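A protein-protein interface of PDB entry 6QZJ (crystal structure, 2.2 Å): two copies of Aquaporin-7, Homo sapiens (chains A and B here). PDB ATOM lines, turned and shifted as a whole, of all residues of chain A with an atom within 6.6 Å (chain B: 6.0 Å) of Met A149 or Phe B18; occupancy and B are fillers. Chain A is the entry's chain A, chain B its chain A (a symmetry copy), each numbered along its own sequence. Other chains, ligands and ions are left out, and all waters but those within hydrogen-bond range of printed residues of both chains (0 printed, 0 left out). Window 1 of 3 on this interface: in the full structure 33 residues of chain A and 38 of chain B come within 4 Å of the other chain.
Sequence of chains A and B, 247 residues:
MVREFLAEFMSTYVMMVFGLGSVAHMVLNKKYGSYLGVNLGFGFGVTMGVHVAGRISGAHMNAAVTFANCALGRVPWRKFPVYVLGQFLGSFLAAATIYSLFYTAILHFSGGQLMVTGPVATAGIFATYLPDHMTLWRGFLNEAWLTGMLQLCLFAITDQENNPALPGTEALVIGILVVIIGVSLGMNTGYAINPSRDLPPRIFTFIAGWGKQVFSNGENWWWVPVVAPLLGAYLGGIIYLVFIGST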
ATOM      1  N   ALA A 144      -6.636  -4.615  26.496  1.00  0.00           N
ATOM      2  CA  ALA A 144      -6.938  -5.495  25.374  1.00  0.00           C
ATOM      3  C   ALA A 144      -5.769  -6.429  25.088  1.00  0.00           C
ATOM      4  O   ALA A 144      -5.953  -7.643  24.945  1.00  0.00           O
ATOM      5  CB  ALA A 144      -7.293  -4.676  24.133  1.00  0.00           C
ATOM      6  N   TRP A 145      -4.553  -5.887  25.023  1.00  0.00           N
ATOM      7  CA  TRP A 145      -3.403  -6.731  24.717  1.00  0.00           C
ATOM      8  C   TRP A 145      -3.129  -7.722  25.842  1.00  0.00           C
ATOM      9  O   TRP A 145      -2.781  -8.879  25.583  1.00  0.00           O
ATOM     10  CB  TRP A 145      -2.168  -5.874  24.439  1.00  0.00           C
ATOM     11  CG  TRP A 145      -1.312  -6.446  23.361  1.00  0.00           C
ATOM     12  CD1 TRP A 145      -0.319  -7.369  23.510  1.00  0.00           C
ATOM     13  CD2 TRP A 145      -1.388  -6.160  21.960  1.00  0.00           C
ATOM     14  NE1 TRP A 145       0.233  -7.674  22.288  1.00  0.00           N
ATOM     15  CE2 TRP A 145      -0.405  -6.943  21.320  1.00  0.00           C
ATOM     16  CE3 TRP A 145      -2.191  -5.320  21.184  1.00  0.00           C
ATOM     17  CZ2 TRP A 145      -0.202  -6.908  19.944  1.00  0.00           C
ATOM     18  CZ3 TRP A 145      -1.986  -5.285  19.815  1.00  0.00           C
ATOM     19  CH2 TRP A 145      -1.000  -6.077  19.210  1.00  0.00           C
ATOM     20  N   LEU A 146      -3.297  -7.295  27.097  1.00  0.00           N
ATOM     21  CA  LEU A 146      -2.976  -8.170  28.219  1.00  0.00           C
ATOM     22  C   LEU A 146      -3.967  -9.323  28.328  1.00  0.00           C
ATOM     23  O   LEU A 146      -3.576 -10.452  28.648  1.00  0.00           O
ATOM     24  CB  LEU A 146      -2.948  -7.371  29.524  1.00  0.00           C
ATOM     25  CG  LEU A 146      -1.631  -6.748  29.993  1.00  0.00           C
ATOM     26  CD1 LEU A 146      -0.858  -6.125  28.839  1.00  0.00           C
ATOM     27  CD2 LEU A 146      -1.909  -5.700  31.074  1.00  0.00           C
ATOM     28  N   THR A 147      -5.256  -9.053  28.101  1.00  0.00           N
ATOM     29  CA  THR A 147      -6.242 -10.127  28.079  1.00  0.00           C
ATOM     30  C   THR A 147      -6.031 -11.040  26.881  1.00  0.00           C
ATOM     31  O   THR A 147      -6.251 -12.252  26.982  1.00  0.00           O
ATOM     32  CB  THR A 147      -7.659  -9.555  28.057  1.00  0.00           C
ATOM     33  OG1 THR A 147      -7.736  -8.427  28.940  1.00  0.00           O
ATOM     34  CG2 THR A 147      -8.660 -10.610  28.503  1.00  0.00           C
ATOM     35  N   GLY A 148      -5.608 -10.477  25.748  1.00  0.00           N
ATOM     36  CA  GLY A 148      -5.240 -11.305  24.614  1.00  0.00           C
ATOM     37  C   GLY A 148      -4.116 -12.269  24.941  1.00  0.00           C
ATOM     38  O   GLY A 148      -4.165 -13.441  24.561  1.00  0.00           O
ATOM     39  N   MET A 149      -3.089 -11.793  25.652  1.00  0.00           N
ATOM     40  CA  MET A 149      -2.030 -12.700  26.085  1.00  0.00           C
ATOM     41  C   MET A 149      -2.589 -13.787  26.995  1.00  0.00           C
ATOM     42  O   MET A 149      -2.184 -14.955  26.906  1.00  0.00           O
ATOM     43  CB  MET A 149      -0.917 -11.928  26.796  1.00  0.00           C
ATOM     44  CG  MET A 149      -0.195 -10.881  25.940  1.00  0.00           C
ATOM     45  SD  MET A 149       1.005 -11.566  24.775  1.00  0.00           S
ATOM     46  CE  MET A 149       2.021 -12.553  25.871  1.00  0.00           C
ATOM     47  N   LEU A 150      -3.532 -13.421  27.870  1.00  0.00           N
ATOM     48  CA  LEU A 150      -4.129 -14.396  28.780  1.00  0.00           C
ATOM     49  C   LEU A 150      -4.889 -15.477  28.014  1.00  0.00           C
ATOM     50  O   LEU A 150      -4.743 -16.670  28.299  1.00  0.00           O
ATOM     51  CB  LEU A 150      -5.055 -13.690  29.772  1.00  0.00           C
ATOM     52  CG  LEU A 150      -5.849 -14.577  30.738  1.00  0.00           C
ATOM     53  CD1 LEU A 150      -4.968 -15.064  31.876  1.00  0.00           C
ATOM     54  CD2 LEU A 150      -7.077 -13.850  31.276  1.00  0.00           C
ATOM     55  N   GLN A 151      -5.701 -15.081  27.032  1.00  0.00           N
ATOM     56  CA  GLN A 151      -6.520 -16.063  26.328  1.00  0.00           C
ATOM     57  C   GLN A 151      -5.671 -16.947  25.421  1.00  0.00           C
ATOM     58  O   GLN A 151      -5.905 -18.159  25.330  1.00  0.00           O
ATOM     59  CB  GLN A 151      -7.614 -15.364  25.525  1.00  0.00           C
ATOM     60  CG  GLN A 151      -8.647 -16.320  24.964  1.00  0.00           C
ATOM     61  CD  GLN A 151      -9.441 -17.008  26.060  1.00  0.00           C
ATOM     62  OE1 GLN A 151     -10.248 -16.375  26.744  1.00  0.00           O
ATOM     63  NE2 GLN A 151      -9.212 -18.304  26.239  1.00  0.00           N
ATOM     64  N   LEU A 152      -4.682 -16.359  24.742  1.00  0.00           N
ATOM     65  CA  LEU A 152      -3.816 -17.146  23.874  1.00  0.00           C
ATOM     66  C   LEU A 152      -3.034 -18.174  24.677  1.00  0.00           C
ATOM     67  O   LEU A 152      -2.922 -19.342  24.276  1.00  0.00           O
ATOM     68  CB  LEU A 152      -2.865 -16.226  23.105  1.00  0.00           C
ATOM     69  CG  LEU A 152      -1.983 -16.948  22.082  1.00  0.00           C
ATOM     70  CD1 LEU A 152      -2.087 -16.304  20.703  1.00  0.00           C
ATOM     71  CD2 LEU A 152      -0.538 -16.980  22.558  1.00  0.00           C
ATOM     72  N   CYS A 153      -2.512 -17.759  25.830  1.00  0.00           N
ATOM     73  CA  CYS A 153      -1.722 -18.644  26.671  1.00  0.00           C
ATOM     74  C   CYS A 153      -2.582 -19.682  27.371  1.00  0.00           C
ATOM     75  O   CYS A 153      -2.128 -20.808  27.607  1.00  0.00           O
ATOM     76  CB  CYS A 153      -0.982 -17.812  27.696  1.00  0.00           C
ATOM     77  SG  CYS A 153       0.426 -17.044  26.912  1.00  0.00           S
ATOM     78  N   LEU A 154      -3.813 -19.312  27.722  1.00  0.00           N
ATOM     79  CA  LEU A 154      -4.746 -20.262  28.311  1.00  0.00           C
ATOM     80  C   LEU A 154      -5.066 -21.398  27.344  1.00  0.00           C
ATOM     81  O   LEU A 154      -5.122 -22.567  27.744  1.00  0.00           O
ATOM     82  CB  LEU A 154      -6.021 -19.530  28.715  1.00  0.00           C
ATOM     83  CG  LEU A 154      -6.247 -19.242  30.196  1.00  0.00           C
ATOM     84  CD1 LEU A 154      -7.461 -18.347  30.374  1.00  0.00           C
ATOM     85  CD2 LEU A 154      -6.432 -20.554  30.950  1.00  0.00           C
ATOM     86  N   LEU A 177       0.896 -18.288  34.772  1.00  0.00           N
ATOM     87  CA  LEU A 177       0.598 -17.319  33.723  1.00  0.00           C
ATOM     88  C   LEU A 177       0.046 -16.017  34.302  1.00  0.00           C
ATOM     89  O   LEU A 177       0.411 -14.923  33.850  1.00  0.00           O
ATOM     90  CB  LEU A 177      -0.389 -17.928  32.729  1.00  0.00           C
ATOM     91  CG  LEU A 177      -1.125 -16.994  31.775  1.00  0.00           C
ATOM     92  CD1 LEU A 177      -0.158 -16.349  30.790  1.00  0.00           C
ATOM     93  CD2 LEU A 177      -2.237 -17.736  31.039  1.00  0.00           C
ATOM     94  N   ILE A 180       2.957 -13.990  35.955  1.00  0.00           N
ATOM     95  CA  ILE A 180       3.869 -13.235  35.100  1.00  0.00           C
ATOM     96  C   ILE A 180       3.158 -12.156  34.298  1.00  0.00           C
ATOM     97  O   ILE A 180       3.809 -11.212  33.833  1.00  0.00           O
ATOM     98  CB  ILE A 180       4.654 -14.163  34.158  1.00  0.00           C
ATOM     99  CG1 ILE A 180       3.702 -15.052  33.355  1.00  0.00           C
ATOM    100  CG2 ILE A 180       5.653 -14.976  34.947  1.00  0.00           C
ATOM    101  CD1 ILE A 180       4.419 -16.010  32.406  1.00  0.00           C
ATOM    102  N   ILE A 181       1.843 -12.268  34.097  1.00  0.00           N
ATOM    103  CA  ILE A 181       1.116 -11.158  33.488  1.00  0.00           C
ATOM    104  C   ILE A 181       1.190  -9.933  34.395  1.00  0.00           C
ATOM    105  O   ILE A 181       1.331  -8.792  33.928  1.00  0.00           O
ATOM    106  CB  ILE A 181      -0.337 -11.569  33.188  1.00  0.00           C
ATOM    107  CG1 ILE A 181      -0.395 -12.477  31.953  1.00  0.00           C
ATOM    108  CG2 ILE A 181      -1.210 -10.348  32.960  1.00  0.00           C
ATOM    109  CD1 ILE A 181      -1.794 -12.796  31.493  1.00  0.00           C
ATOM    110  N   GLY A 182       1.110 -10.154  35.710  1.00  0.00           N
ATOM    111  CA  GLY A 182       1.328  -9.064  36.647  1.00  0.00           C
ATOM    112  C   GLY A 182       2.767  -8.593  36.667  1.00  0.00           C
ATOM    113  O   GLY A 182       3.037  -7.391  36.554  1.00  0.00           O
ATOM    114  N   VAL A 183       3.711  -9.529  36.794  1.00  0.00           N
ATOM    115  CA  VAL A 183       5.120  -9.153  36.875  1.00  0.00           C
ATOM    116  C   VAL A 183       5.538  -8.357  35.643  1.00  0.00           C
ATOM    117  O   VAL A 183       6.186  -7.310  35.756  1.00  0.00           O
ATOM    118  CB  VAL A 183       6.006 -10.399  37.070  1.00  0.00           C
ATOM    119  CG1 VAL A 183       7.467 -10.034  36.869  1.00  0.00           C
ATOM    120  CG2 VAL A 183       5.800 -10.991  38.454  1.00  0.00           C
ATOM    121  N   SER A 184       5.130  -8.807  34.453  1.00  0.00           N
ATOM    122  CA  SER A 184       5.649  -8.256  33.206  1.00  0.00           C
ATOM    123  C   SER A 184       4.797  -7.150  32.594  1.00  0.00           C
ATOM    124  O   SER A 184       5.296  -6.416  31.735  1.00  0.00           O
ATOM    125  CB  SER A 184       5.807  -9.364  32.159  1.00  0.00           C
ATOM    126  OG  SER A 184       6.768 -10.324  32.561  1.00  0.00           O
ATOM    127  N   LEU A 185       3.526  -7.021  32.977  1.00  0.00           N
ATOM    128  CA  LEU A 185       2.649  -6.104  32.258  1.00  0.00           C
ATOM    129  C   LEU A 185       1.668  -5.357  33.157  1.00  0.00           C
ATOM    130  O   LEU A 185       0.767  -4.691  32.636  1.00  0.00           O
ATOM    131  CB  LEU A 185       1.866  -6.868  31.170  1.00  0.00           C
ATOM    132  CG  LEU A 185       2.658  -7.590  30.073  1.00  0.00           C
ATOM    133  CD1 LEU A 185       1.799  -8.620  29.341  1.00  0.00           C
ATOM    134  CD2 LEU A 185       3.245  -6.582  29.092  1.00  0.00           C
ATOM    135  N   GLY A 232     -10.076  -8.097  23.932  1.00  0.00           N
ATOM    136  CA  GLY A 232      -8.765  -8.718  24.027  1.00  0.00           C
ATOM    137  C   GLY A 232      -8.836 -10.235  24.044  1.00  0.00           C
ATOM    138  O   GLY A 232      -8.155 -10.907  23.264  1.00  0.00           O
ATOM    139  N   GLY A 236      -7.228 -12.571  21.280  1.00  0.00           N
ATOM    140  CA  GLY A 236      -6.206 -13.538  21.644  1.00  0.00           C
ATOM    141  C   GLY A 236      -6.575 -14.965  21.273  1.00  0.00           C
ATOM    142  O   GLY A 236      -5.740 -15.717  20.763  1.00  0.00           O
ATOM    143  N   TYR B  13       7.479 -14.627  20.310  1.00  0.00           N
ATOM    144  CA  TYR B  13       6.740 -13.401  20.593  1.00  0.00           C
ATOM    145  C   TYR B  13       6.216 -13.401  22.024  1.00  0.00           C
ATOM    146  O   TYR B  13       6.424 -12.441  22.776  1.00  0.00           O
ATOM    147  CB  TYR B  13       5.585 -13.232  19.607  1.00  0.00           C
ATOM    148  CG  TYR B  13       4.723 -12.029  19.912  1.00  0.00           C
ATOM    149  CD1 TYR B  13       3.509 -12.165  20.582  1.00  0.00           C
ATOM    150  CD2 TYR B  13       5.133 -10.746  19.545  1.00  0.00           C
ATOM    151  CE1 TYR B  13       2.725 -11.057  20.868  1.00  0.00           C
ATOM    152  CE2 TYR B  13       4.355  -9.638  19.824  1.00  0.00           C
ATOM    153  CZ  TYR B  13       3.157  -9.797  20.487  1.00  0.00           C
ATOM    154  OH  TYR B  13       2.384  -8.694  20.764  1.00  0.00           O
ATOM    155  N   VAL B  14       5.533 -14.476  22.412  1.00  0.00           N
ATOM    156  CA  VAL B  14       4.982 -14.572  23.760  1.00  0.00           C
ATOM    157  C   VAL B  14       6.094 -14.507  24.799  1.00  0.00           C
ATOM    158  O   VAL B  14       5.980 -13.798  25.806  1.00  0.00           O
ATOM    159  CB  VAL B  14       4.146 -15.860  23.896  1.00  0.00           C
ATOM    160  CG1 VAL B  14       3.758 -16.100  25.340  1.00  0.00           C
ATOM    161  CG2 VAL B  14       2.909 -15.782  23.012  1.00  0.00           C
ATOM    162  N   MET B  15       7.191 -15.233  24.566  1.00  0.00           N
ATOM    163  CA  MET B  15       8.291 -15.246  25.525  1.00  0.00           C
ATOM    164  C   MET B  15       8.872 -13.852  25.718  1.00  0.00           C
ATOM    165  O   MET B  15       9.164 -13.445  26.849  1.00  0.00           O
ATOM    166  CB  MET B  15       9.384 -16.212  25.067  1.00  0.00           C
ATOM    167  CG  MET B  15      10.590 -16.278  25.996  1.00  0.00           C
ATOM    168  SD  MET B  15      11.914 -15.127  25.548  1.00  0.00           S
ATOM    169  CE  MET B  15      12.494 -15.840  24.006  1.00  0.00           C
ATOM    170  N   MET B  16       9.056 -13.112  24.626  1.00  0.00           N
ATOM    171  CA  MET B  16       9.707 -11.811  24.718  1.00  0.00           C
ATOM    172  C   MET B  16       8.781 -10.744  25.291  1.00  0.00           C
ATOM    173  O   MET B  16       9.257  -9.794  25.918  1.00  0.00           O
ATOM    174  CB  MET B  16      10.233 -11.401  23.345  1.00  0.00           C
ATOM    175  CG  MET B  16      11.366 -12.280  22.837  1.00  0.00           C
ATOM    176  SD  MET B  16      12.895 -12.093  23.784  1.00  0.00           S
ATOM    177  CE  MET B  16      13.297 -10.384  23.409  1.00  0.00           C
ATOM    178  N   VAL B  17       7.466 -10.884  25.108  1.00  0.00           N
ATOM    179  CA  VAL B  17       6.535  -9.944  25.728  1.00  0.00           C
ATOM    180  C   VAL B  17       6.632 -10.035  27.247  1.00  0.00           C
ATOM    181  O   VAL B  17       6.789  -9.020  27.937  1.00  0.00           O
ATOM    182  CB  VAL B  17       5.098 -10.196  25.232  1.00  0.00           C
ATOM    183  CG1 VAL B  17       4.096  -9.488  26.133  1.00  0.00           C
ATOM    184  CG2 VAL B  17       4.943  -9.728  23.791  1.00  0.00           C
ATOM    185  N   PHE B  18       6.548 -11.258  27.788  1.00  0.00           N
ATOM    186  CA  PHE B  18       6.742 -11.446  29.223  1.00  0.00           C
ATOM    187  C   PHE B  18       8.152 -11.065  29.652  1.00  0.00           C
ATOM    188  O   PHE B  18       8.347 -10.551  30.759  1.00  0.00           O
ATOM    189  CB  PHE B  18       6.454 -12.902  29.622  1.00  0.00           C
ATOM    190  CG  PHE B  18       4.996 -13.277  29.559  1.00  0.00           C
ATOM    191  CD1 PHE B  18       4.064 -12.647  30.373  1.00  0.00           C
ATOM    192  CD2 PHE B  18       4.558 -14.252  28.678  1.00  0.00           C
ATOM    193  CE1 PHE B  18       2.721 -12.992  30.307  1.00  0.00           C
ATOM    194  CE2 PHE B  18       3.217 -14.605  28.612  1.00  0.00           C
ATOM    195  CZ  PHE B  18       2.298 -13.974  29.421  1.00  0.00           C
ATOM    196  N   GLY B  19       9.147 -11.308  28.801  1.00  0.00           N
ATOM    197  CA  GLY B  19      10.507 -10.950  29.144  1.00  0.00           C
ATOM    198  C   GLY B  19      10.729  -9.448  29.189  1.00  0.00           C
ATOM    199  O   GLY B  19      10.987  -8.877  30.257  1.00  0.00           O
ATOM    200  N   LEU B  20      10.612  -8.795  28.030  1.00  0.00           N
ATOM    201  CA  LEU B  20      10.921  -7.371  27.946  1.00  0.00           C
ATOM    202  C   LEU B  20       9.977  -6.533  28.800  1.00  0.00           C
ATOM    203  O   LEU B  20      10.347  -5.439  29.242  1.00  0.00           O
ATOM    204  CB  LEU B  20      10.880  -6.920  26.486  1.00  0.00           C
ATOM    205  CG  LEU B  20      11.925  -7.580  25.583  1.00  0.00           C
ATOM    206  CD1 LEU B  20      11.929  -6.943  24.201  1.00  0.00           C
ATOM    207  CD2 LEU B  20      13.319  -7.517  26.211  1.00  0.00           C
ATOM    208  N   GLY B  21       8.758  -7.020  29.036  1.00  0.00           N
ATOM    209  CA  GLY B  21       7.867  -6.327  29.951  1.00  0.00           C
ATOM    210  C   GLY B  21       8.368  -6.363  31.383  1.00  0.00           C
ATOM    211  O   GLY B  21       8.244  -5.378  32.118  1.00  0.00           O
ATOM    212  N   SER B  22       8.941  -7.498  31.803  1.00  0.00           N
ATOM    213  CA  SER B  22       9.511  -7.583  33.145  1.00  0.00           C
ATOM    214  C   SER B  22      10.680  -6.619  33.302  1.00  0.00           C
ATOM    215  O   SER B  22      10.806  -5.955  34.338  1.00  0.00           O
ATOM    216  CB  SER B  22       9.948  -9.020  33.456  1.00  0.00           C
ATOM    217  OG  SER B  22      11.084  -9.391  32.695  1.00  0.00           O
ATOM    218  N   VAL B  23      11.531  -6.516  32.276  1.00  0.00           N
ATOM    219  CA  VAL B  23      12.673  -5.609  32.343  1.00  0.00           C
ATOM    220  C   VAL B  23      12.207  -4.162  32.362  1.00  0.00           C
ATOM    221  O   VAL B  23      12.772  -3.325  33.075  1.00  0.00           O
ATOM    222  CB  VAL B  23      13.639  -5.875  31.176  1.00  0.00           C
ATOM    223  CG1 VAL B  23      14.884  -5.002  31.296  1.00  0.00           C
ATOM    224  CG2 VAL B  23      14.020  -7.361  31.122  1.00  0.00           C
ATOM    225  N   GLY B  37      11.784 -10.192  39.450  1.00  0.00           N
ATOM    226  CA  GLY B  37      10.715 -10.171  38.467  1.00  0.00           C
ATOM    227  C   GLY B  37      11.209 -10.325  37.042  1.00  0.00           C
ATOM    228  O   GLY B  37      10.546 -10.966  36.222  1.00  0.00           O
ATOM    229  N   GLY B  41       9.930 -13.158  34.858  1.00  0.00           N
ATOM    230  CA  GLY B  41       9.228 -12.812  33.633  1.00  0.00           C
ATOM    231  C   GLY B  41       9.793 -13.514  32.414  1.00  0.00           C
ATOM    232  O   GLY B  41       9.044 -14.003  31.566  1.00  0.00           O
ATOM    233  N   PHE B  42      11.124 -13.581  32.312  1.00  0.00           N
ATOM    234  CA  PHE B  42      11.752 -14.297  31.207  1.00  0.00           C
ATOM    235  C   PHE B  42      11.684 -15.808  31.408  1.00  0.00           C
ATOM    236  O   PHE B  42      11.426 -16.554  30.458  1.00  0.00           O
ATOM    237  CB  PHE B  42      13.205 -13.859  31.056  1.00  0.00           C
ATOM    238  CG  PHE B  42      13.428 -12.808  29.994  1.00  0.00           C
ATOM    239  CD1 PHE B  42      13.318 -13.122  28.648  1.00  0.00           C
ATOM    240  CD2 PHE B  42      13.782 -11.512  30.351  1.00  0.00           C
ATOM    241  CE1 PHE B  42      13.536 -12.163  27.678  1.00  0.00           C
ATOM    242  CE2 PHE B  42      14.005 -10.545  29.386  1.00  0.00           C
ATOM    243  CZ  PHE B  42      13.879 -10.869  28.046  1.00  0.00           C
ATOM    244  N   PHE B  44       9.452 -17.866  33.275  1.00  0.00           N
ATOM    245  CA  PHE B  44       8.144 -18.442  33.005  1.00  0.00           C
ATOM    246  C   PHE B  44       7.537 -17.921  31.709  1.00  0.00           C
ATOM    247  O   PHE B  44       6.591 -18.535  31.201  1.00  0.00           O
ATOM    248  CB  PHE B  44       7.226 -18.204  34.205  1.00  0.00           C
ATOM    249  CG  PHE B  44       7.637 -18.986  35.430  1.00  0.00           C
ATOM    250  CD1 PHE B  44       7.659 -20.379  35.402  1.00  0.00           C
ATOM    251  CD2 PHE B  44       8.023 -18.338  36.595  1.00  0.00           C
ATOM    252  CE1 PHE B  44       8.038 -21.111  36.518  1.00  0.00           C
ATOM    253  CE2 PHE B  44       8.413 -19.056  37.718  1.00  0.00           C
ATOM    254  CZ  PHE B  44       8.425 -20.444  37.680  1.00  0.00           C
ATOM    255  N   GLY B  45       8.073 -16.833  31.146  1.00  0.00           N
ATOM    256  CA  GLY B  45       7.765 -16.509  29.764  1.00  0.00           C
ATOM    257  C   GLY B  45       8.203 -17.608  28.809  1.00  0.00           C
ATOM    258  O   GLY B  45       7.511 -17.910  27.832  1.00  0.00           O
ATOM    259  N   MET B  48       5.645 -20.425  28.852  1.00  0.00           N
ATOM    260  CA  MET B  48       4.459 -20.258  28.015  1.00  0.00           C
ATOM    261  C   MET B  48       4.776 -20.532  26.550  1.00  0.00           C
ATOM    262  O   MET B  48       3.980 -21.167  25.846  1.00  0.00           O
ATOM    263  CB  MET B  48       3.878 -18.855  28.194  1.00  0.00           C
ATOM    264  CG  MET B  48       3.480 -18.540  29.629  1.00  0.00           C
ATOM    265  SD  MET B  48       2.354 -19.764  30.325  1.00  0.00           S
ATOM    266  CE  MET B  48       2.853 -19.752  32.047  1.00  0.00           C
ATOM    267  N   ILE B  98       5.998  -3.960  23.482  1.00  0.00           N
ATOM    268  CA  ILE B  98       6.304  -3.372  24.781  1.00  0.00           C
ATOM    269  C   ILE B  98       6.496  -1.862  24.655  1.00  0.00           C
ATOM    270  O   ILE B  98       6.046  -1.091  25.510  1.00  0.00           O
ATOM    271  CB  ILE B  98       7.539  -4.061  25.391  1.00  0.00           C
ATOM    272  CG1 ILE B  98       7.285  -5.565  25.576  1.00  0.00           C
ATOM    273  CG2 ILE B  98       7.918  -3.417  26.708  1.00  0.00           C
ATOM    274  CD1 ILE B  98       6.157  -5.898  26.546  1.00  0.00           C
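No position is printed for both chains.
Of the printed residues of chain B, Met A149 touches Val B14 (3.99 Å), Val B17 (3.7 Å) and Phe B18 (3.6 Å). Printed residues of chain A within 4 Å of Phe B18: Met A149 (3.6 Å), Leu A177 (3.7 Å), Ile A180 (3.8 Å), Ile A181 (3.6 Å) and Ser A184 (2.4 Å). Printed residues of chain A within 4 Å of Gly B45: Ile A180. Of the printed residues of chain A, Val B17 touches Met A149. Of the printed residues of chain A, Gly B37 touches Val A183. Of the printed residues of chain B, Trp A145 touches Tyr B13 (2.8 Å). Phe B42 touches none of the printed residues of chain A. The nearest residue of chain A that does not touch Phe B18 is Cys A153 (4.1 Å).
NE1 of Trp A145 is in hydrogen-bond range of OH of Tyr B13, 2.8 Å away. The side-chain hydroxyl (OG) of Ser A184 sits at hydrogen-bond distance from the backbone carbonyl oxygen (O) of Phe B18 (2.4 Å). O of Gly B21 lies close to O of Ser A184.
Hydrophobic or aromatic side chains of chain A within 4 Å of the printed part of chain B: Trp A145, Met A149, Leu A152, Leu A177, Ile A180, Ile A181, Val A183 and Leu A185. Of the 18 printed residues of chain B, 12 touch a printed residue of chain A. Among the printed residues, 19 pairs touch across the chains.
CG1 of Val B17 touches CE of Met A149, 3.7 Å away. Met A149 touches Phe B18 (CE to CE2, 3.6 Å). SG of Cys A153 touches CG1 of Val B14, at 3.8 Å. CD1 of Leu A177 touches CZ of Phe B18, at 3.7 Å. O of Ile A180 touches CD1 of Phe B18, 3.8 Å away. O of Phe B44 touches CD1 of Ile A180, 3.5 Å away. Ile A180 touches Gly B45. Ile A180 touches Met B48 (CD1 to CG, 3.9 Å). Gly B41 touches Ser A184 (CA to OG, 3.7 Å). Leu A185 touches Ile B98 (CD2 to CD1, 3.9 Å).
O of Met A149 sits close to SG of Cys A153, 3.3 Å away. The backbone carbonyl oxygen (O) of Ile A180 sits close to the side-chain hydroxyl (OG) of Ser A184 (3.3 Å). The backbone carbonyl oxygen of Gly B19 is in hydrogen-bond range of the side-chain hydroxyl of Ser B22.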
